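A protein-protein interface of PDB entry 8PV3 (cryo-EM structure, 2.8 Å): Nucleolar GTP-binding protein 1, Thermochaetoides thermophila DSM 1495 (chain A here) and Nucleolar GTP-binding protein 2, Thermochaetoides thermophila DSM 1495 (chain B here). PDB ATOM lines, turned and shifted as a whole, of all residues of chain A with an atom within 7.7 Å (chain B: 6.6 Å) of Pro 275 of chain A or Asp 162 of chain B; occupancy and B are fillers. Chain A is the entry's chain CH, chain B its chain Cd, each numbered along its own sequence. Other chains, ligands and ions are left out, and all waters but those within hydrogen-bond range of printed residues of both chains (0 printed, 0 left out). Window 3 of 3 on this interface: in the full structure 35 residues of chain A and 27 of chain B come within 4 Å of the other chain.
OG of Ser 272 of chain A is in hydrogen-bond range of O of Leu 269 of chain A (2.7 Å). OE1 of Glu 163 of chain B sits at hydrogen-bond distance from N of Thr 160 of chain B (3.0 Å).
Among the printed residues, merely in contact across the chains: Ser 272 of chain A with Val 161 of chain B, Pro 275 of chain A with Asp 162 of chain B, Leu 228 of chain A with Thr 160 of chain B, Leu 276 of chain A with Val 161 of chain B, Pro 275 of chain A with Val 161 of chain B, Pro 275 of chain A with Ala 165 of chain B and Leu 276 of chain A with Leu 164 of chain B.
Of chain B, only Val 161, Asp 162 and Ala 165 come within 4 Å of Pro 275 of chain A. Asp 162 of chain B touches just one residue of chain A: Pro 275 (3.5 Å). Of the printed residues of chain A, Thr 160 of chain B touches Leu 228 (3.5 Å). Printed residues of chain A within 4 Å of Ala 165 of chain B: Pro 275. Of the printed residues of chain B, Leu 228 of chain A touches Thr 160 (3.5 Å). Ile 273 of chain A touches none of the printed residues of chain B.
Hydrophobic or aromatic side chains of chain A within 4 Å of the printed part of chain B: Leu 228, Pro 275 and Leu 276.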
ATOM      1  N   LEU A 228      17.828  -9.346  25.456  1.00  0.00           N
ATOM      2  CA  LEU A 228      17.425 -10.738  25.646  1.00  0.00           C
ATOM      3  C   LEU A 228      16.245 -10.872  26.599  1.00  0.00           C
ATOM      4  O   LEU A 228      15.522 -11.875  26.564  1.00  0.00           O
ATOM      5  CB  LEU A 228      18.606 -11.555  26.166  1.00  0.00           C
ATOM      6  CG  LEU A 228      19.914 -11.489  25.382  1.00  0.00           C
ATOM      7  CD1 LEU A 228      21.006 -12.201  26.154  1.00  0.00           C
ATOM      8  CD2 LEU A 228      19.741 -12.102  24.006  1.00  0.00           C
ATOM      9  N   LEU A 242      22.536 -19.571  17.335  1.00  0.00           N
ATOM     10  CA  LEU A 242      23.717 -18.744  17.112  1.00  0.00           C
ATOM     11  C   LEU A 242      24.725 -18.871  18.244  1.00  0.00           C
ATOM     12  O   LEU A 242      25.932 -18.757  18.010  1.00  0.00           O
ATOM     13  CB  LEU A 242      23.320 -17.281  16.938  1.00  0.00           C
ATOM     14  CG  LEU A 242      22.598 -16.869  15.660  1.00  0.00           C
ATOM     15  CD1 LEU A 242      22.001 -15.494  15.840  1.00  0.00           C
ATOM     16  CD2 LEU A 242      23.554 -16.883  14.491  1.00  0.00           C
ATOM     17  N   LEU A 269      21.485  -4.565  15.074  1.00  0.00           N
ATOM     18  CA  LEU A 269      21.302  -5.955  15.480  1.00  0.00           C
ATOM     19  C   LEU A 269      22.549  -6.777  15.185  1.00  0.00           C
ATOM     20  O   LEU A 269      22.936  -7.646  15.979  1.00  0.00           O
ATOM     21  CB  LEU A 269      20.083  -6.565  14.787  1.00  0.00           C
ATOM     22  CG  LEU A 269      19.809  -8.028  15.161  1.00  0.00           C
ATOM     23  CD1 LEU A 269      19.710  -8.199  16.673  1.00  0.00           C
ATOM     24  CD2 LEU A 269      18.574  -8.581  14.484  1.00  0.00           C
ATOM     25  N   PHE A 270      23.194  -6.515  14.041  1.00  0.00           N
ATOM     26  CA  PHE A 270      24.450  -7.196  13.732  1.00  0.00           C
ATOM     27  C   PHE A 270      25.519  -6.871  14.769  1.00  0.00           C
ATOM     28  O   PHE A 270      26.222  -7.766  15.257  1.00  0.00           O
ATOM     29  CB  PHE A 270      24.921  -6.813  12.331  1.00  0.00           C
ATOM     30  CG  PHE A 270      26.145  -7.555  11.880  1.00  0.00           C
ATOM     31  CD1 PHE A 270      26.041  -8.832  11.359  1.00  0.00           C
ATOM     32  CD2 PHE A 270      27.398  -6.975  11.971  1.00  0.00           C
ATOM     33  CE1 PHE A 270      27.163  -9.517  10.944  1.00  0.00           C
ATOM     34  CE2 PHE A 270      28.522  -7.656  11.557  1.00  0.00           C
ATOM     35  CZ  PHE A 270      28.404  -8.928  11.042  1.00  0.00           C
ATOM     36  N   LYS A 271      25.632  -5.594  15.144  1.00  0.00           N
ATOM     37  CA  LYS A 271      26.609  -5.200  16.155  1.00  0.00           C
ATOM     38  C   LYS A 271      26.261  -5.771  17.526  1.00  0.00           C
ATOM     39  O   LYS A 271      27.154  -6.040  18.338  1.00  0.00           O
ATOM     40  CB  LYS A 271      26.711  -3.678  16.226  1.00  0.00           C
ATOM     41  CG  LYS A 271      27.308  -3.025  14.993  1.00  0.00           C
ATOM     42  CD  LYS A 271      27.308  -1.513  15.133  1.00  0.00           C
ATOM     43  CE  LYS A 271      27.995  -0.846  13.955  1.00  0.00           C
ATOM     44  NZ  LYS A 271      27.867   0.637  14.007  1.00  0.00           N
ATOM     45  N   SER A 272      24.970  -5.958  17.803  1.00  0.00           N
ATOM     46  CA  SER A 272      24.564  -6.486  19.101  1.00  0.00           C
ATOM     47  C   SER A 272      24.857  -7.975  19.214  1.00  0.00           C
ATOM     48  O   SER A 272      25.307  -8.446  20.265  1.00  0.00           O
ATOM     49  CB  SER A 272      23.081  -6.214  19.337  1.00  0.00           C
ATOM     50  OG  SER A 272      22.282  -6.991  18.464  1.00  0.00           O
ATOM     51  N   ILE A 273      24.605  -8.741  18.145  1.00  0.00           N
ATOM     52  CA  ILE A 273      24.856 -10.180  18.193  1.00  0.00           C
ATOM     53  C   ILE A 273      26.253 -10.548  17.715  1.00  0.00           C
ATOM     54  O   ILE A 273      26.559 -11.742  17.597  1.00  0.00           O
ATOM     55  CB  ILE A 273      23.816 -10.977  17.378  1.00  0.00           C
ATOM     56  CG1 ILE A 273      23.975 -10.713  15.881  1.00  0.00           C
ATOM     57  CG2 ILE A 273      22.411 -10.640  17.848  1.00  0.00           C
ATOM     58  CD1 ILE A 273      22.895 -11.349  15.036  1.00  0.00           C
ATOM     59  N   LYS A 274      27.098  -9.560  17.415  1.00  0.00           N
ATOM     60  CA  LYS A 274      28.501  -9.839  17.112  1.00  0.00           C
ATOM     61  C   LYS A 274      29.274 -10.620  18.184  1.00  0.00           C
ATOM     62  O   LYS A 274      30.081 -11.480  17.793  1.00  0.00           O
ATOM     63  CB  LYS A 274      29.214  -8.518  16.781  1.00  0.00           C
ATOM     64  CG  LYS A 274      30.618  -8.680  16.227  1.00  0.00           C
ATOM     65  CD  LYS A 274      31.163  -7.360  15.712  1.00  0.00           C
ATOM     66  CE  LYS A 274      31.561  -6.445  16.856  1.00  0.00           C
ATOM     67  NZ  LYS A 274      32.249  -5.219  16.368  1.00  0.00           N
ATOM     68  N   PRO A 275      29.129 -10.381  19.504  1.00  0.00           N
ATOM     69  CA  PRO A 275      29.912 -11.196  20.459  1.00  0.00           C
ATOM     70  C   PRO A 275      29.589 -12.687  20.468  1.00  0.00           C
ATOM     71  O   PRO A 275      30.419 -13.475  20.937  1.00  0.00           O
ATOM     72  CB  PRO A 275      29.595 -10.551  21.811  1.00  0.00           C
ATOM     73  CG  PRO A 275      29.276  -9.163  21.491  1.00  0.00           C
ATOM     74  CD  PRO A 275      28.529  -9.223  20.199  1.00  0.00           C
ATOM     75  N   LEU A 276      28.419 -13.109  19.976  1.00  0.00           N
ATOM     76  CA  LEU A 276      28.182 -14.536  19.775  1.00  0.00           C
ATOM     77  C   LEU A 276      29.033 -15.120  18.658  1.00  0.00           C
ATOM     78  O   LEU A 276      29.193 -16.342  18.594  1.00  0.00           O
ATOM     79  CB  LEU A 276      26.711 -14.824  19.454  1.00  0.00           C
ATOM     80  CG  LEU A 276      25.652 -14.951  20.554  1.00  0.00           C
ATOM     81  CD1 LEU A 276      25.311 -13.628  21.151  1.00  0.00           C
ATOM     82  CD2 LEU A 276      24.397 -15.585  19.998  1.00  0.00           C
ATOM     83  N   PHE A 277      29.580 -14.279  17.786  1.00  0.00           N
ATOM     84  CA  PHE A 277      30.279 -14.737  16.594  1.00  0.00           C
ATOM     85  C   PHE A 277      31.763 -14.965  16.824  1.00  0.00           C
ATOM     86  O   PHE A 277      32.495 -15.170  15.850  1.00  0.00           O
ATOM     87  CB  PHE A 277      30.088 -13.736  15.456  1.00  0.00           C
ATOM     88  CG  PHE A 277      28.657 -13.554  15.036  1.00  0.00           C
ATOM     89  CD1 PHE A 277      27.717 -14.552  15.246  1.00  0.00           C
ATOM     90  CD2 PHE A 277      28.251 -12.376  14.433  1.00  0.00           C
ATOM     91  CE1 PHE A 277      26.406 -14.377  14.865  1.00  0.00           C
ATOM     92  CE2 PHE A 277      26.939 -12.197  14.046  1.00  0.00           C
ATOM     93  CZ  PHE A 277      26.017 -13.200  14.261  1.00  0.00           C
ATOM     94  N   ALA A 278      32.226 -14.898  18.070  1.00  0.00           N
ATOM     95  CA  ALA A 278      33.597 -15.279  18.377  1.00  0.00           C
ATOM     96  C   ALA A 278      33.805 -16.756  18.069  1.00  0.00           C
ATOM     97  O   ALA A 278      32.926 -17.590  18.303  1.00  0.00           O
ATOM     98  CB  ALA A 278      33.918 -14.993  19.842  1.00  0.00           C
ATOM     99  N   ASN A 279      34.977 -17.064  17.508  1.00  0.00           N
ATOM    100  CA  ASN A 279      35.369 -18.375  16.992  1.00  0.00           C
ATOM    101  C   ASN A 279      34.447 -18.873  15.887  1.00  0.00           C
ATOM    102  O   ASN A 279      34.361 -20.088  15.665  1.00  0.00           O
ATOM    103  CB  ASN A 279      35.458 -19.432  18.100  1.00  0.00           C
ATOM    104  CG  ASN A 279      36.529 -19.114  19.115  1.00  0.00           C
ATOM    105  OD1 ASN A 279      36.237 -18.855  20.283  1.00  0.00           O
ATOM    106  ND2 ASN A 279      37.781 -19.129  18.677  1.00  0.00           N
ATOM    107  N   LYS A 280      33.756 -17.976  15.185  1.00  0.00           N
ATOM    108  CA  LYS A 280      32.866 -18.350  14.096  1.00  0.00           C
ATOM    109  C   LYS A 280      33.108 -17.445  12.897  1.00  0.00           C
ATOM    110  O   LYS A 280      33.799 -16.427  12.979  1.00  0.00           O
ATOM    111  CB  LYS A 280      31.383 -18.299  14.504  1.00  0.00           C
ATOM    112  CG  LYS A 280      31.025 -19.183  15.688  1.00  0.00           C
ATOM    113  CD  LYS A 280      29.551 -19.106  16.042  1.00  0.00           C
ATOM    114  CE  LYS A 280      29.270 -19.907  17.302  1.00  0.00           C
ATOM    115  NZ  LYS A 280      27.821 -20.060  17.574  1.00  0.00           N
ATOM    116  N   THR B 160      22.857 -10.756  29.444  1.00  0.00           N
ATOM    117  CA  THR B 160      23.482  -9.982  28.384  1.00  0.00           C
ATOM    118  C   THR B 160      24.112 -10.901  27.347  1.00  0.00           C
ATOM    119  O   THR B 160      24.234 -12.115  27.535  1.00  0.00           O
ATOM    120  CB  THR B 160      24.558  -9.022  28.920  1.00  0.00           C
ATOM    121  OG1 THR B 160      25.736  -9.762  29.261  1.00  0.00           O
ATOM    122  CG2 THR B 160      24.065  -8.264  30.143  1.00  0.00           C
ATOM    123  N   VAL B 161      24.519 -10.275  26.242  1.00  0.00           N
ATOM    124  CA  VAL B 161      25.133 -10.978  25.120  1.00  0.00           C
ATOM    125  C   VAL B 161      26.474 -11.587  25.523  1.00  0.00           C
ATOM    126  O   VAL B 161      26.784 -12.739  25.180  1.00  0.00           O
ATOM    127  CB  VAL B 161      25.271  -9.998  23.939  1.00  0.00           C
ATOM    128  CG1 VAL B 161      26.103 -10.578  22.840  1.00  0.00           C
ATOM    129  CG2 VAL B 161      23.895  -9.616  23.415  1.00  0.00           C
ATOM    130  N   ASP B 162      27.291 -10.823  26.254  1.00  0.00           N
ATOM    131  CA  ASP B 162      28.588 -11.324  26.702  1.00  0.00           C
ATOM    132  C   ASP B 162      28.427 -12.466  27.696  1.00  0.00           C
ATOM    133  O   ASP B 162      29.191 -13.441  27.663  1.00  0.00           O
ATOM    134  CB  ASP B 162      29.401 -10.187  27.317  1.00  0.00           C
ATOM    135  CG  ASP B 162      29.852  -9.172  26.290  1.00  0.00           C
ATOM    136  OD1 ASP B 162      30.049  -9.558  25.120  1.00  0.00           O
ATOM    137  OD2 ASP B 162      30.002  -7.986  26.651  1.00  0.00           O
ATOM    138  N   GLU B 163      27.439 -12.359  28.590  1.00  0.00           N
ATOM    139  CA  GLU B 163      27.141 -13.454  29.505  1.00  0.00           C
ATOM    140  C   GLU B 163      26.682 -14.693  28.755  1.00  0.00           C
ATOM    141  O   GLU B 163      27.035 -15.810  29.140  1.00  0.00           O
ATOM    142  CB  GLU B 163      26.076 -13.032  30.517  1.00  0.00           C
ATOM    143  CG  GLU B 163      26.537 -11.992  31.517  1.00  0.00           C
ATOM    144  CD  GLU B 163      25.386 -11.402  32.304  1.00  0.00           C
ATOM    145  OE1 GLU B 163      24.222 -11.709  31.975  1.00  0.00           O
ATOM    146  OE2 GLU B 163      25.644 -10.630  33.252  1.00  0.00           O
ATOM    147  N   LEU B 164      25.904 -14.512  27.683  1.00  0.00           N
ATOM    148  CA  LEU B 164      25.491 -15.642  26.856  1.00  0.00           C
ATOM    149  C   LEU B 164      26.685 -16.334  26.212  1.00  0.00           C
ATOM    150  O   LEU B 164      26.775 -17.569  26.224  1.00  0.00           O
ATOM    151  CB  LEU B 164      24.519 -15.164  25.781  1.00  0.00           C
ATOM    152  CG  LEU B 164      24.099 -16.146  24.689  1.00  0.00           C
ATOM    153  CD1 LEU B 164      23.559 -17.451  25.251  1.00  0.00           C
ATOM    154  CD2 LEU B 164      23.084 -15.482  23.794  1.00  0.00           C
ATOM    155  N   ALA B 165      27.609 -15.552  25.641  1.00  0.00           N
ATOM    156  CA  ALA B 165      28.785 -16.140  25.000  1.00  0.00           C
ATOM    157  C   ALA B 165      29.658 -16.879  26.010  1.00  0.00           C
ATOM    158  O   ALA B 165      30.084 -18.021  25.764  1.00  0.00           O
ATOM    159  CB  ALA B 165      29.588 -15.055  24.287  1.00  0.00           C
ATOM    160  N   GLY B 166      29.896 -16.259  27.170  1.00  0.00           N
ATOM    161  CA  GLY B 166      30.670 -16.919  28.206  1.00  0.00           C
ATOM    162  C   GLY B 166      30.012 -18.189  28.709  1.00  0.00           C
ATOM    163  O   GLY B 166      30.665 -19.231  28.807  1.00  0.00           O
ATOM    164  N   TYR B 167      28.701 -18.128  28.978  1.00  0.00           N
ATOM    165  CA  TYR B 167      27.961 -19.278  29.484  1.00  0.00           C
ATOM    166  C   TYR B 167      27.965 -20.423  28.486  1.00  0.00           C
ATOM    167  O   TYR B 167      28.066 -21.589  28.882  1.00  0.00           O
ATOM    168  CB  TYR B 167      26.531 -18.856  29.835  1.00  0.00           C
ATOM    169  CG  TYR B 167      25.516 -19.980  29.892  1.00  0.00           C
ATOM    170  CD1 TYR B 167      25.347 -20.727  31.049  1.00  0.00           C
ATOM    171  CD2 TYR B 167      24.688 -20.257  28.806  1.00  0.00           C
ATOM    172  CE1 TYR B 167      24.416 -21.743  31.112  1.00  0.00           C
ATOM    173  CE2 TYR B 167      23.757 -21.273  28.861  1.00  0.00           C
ATOM    174  CZ  TYR B 167      23.624 -22.010  30.017  1.00  0.00           C
ATOM    175  OH  TYR B 167      22.694 -23.019  30.078  1.00  0.00           O
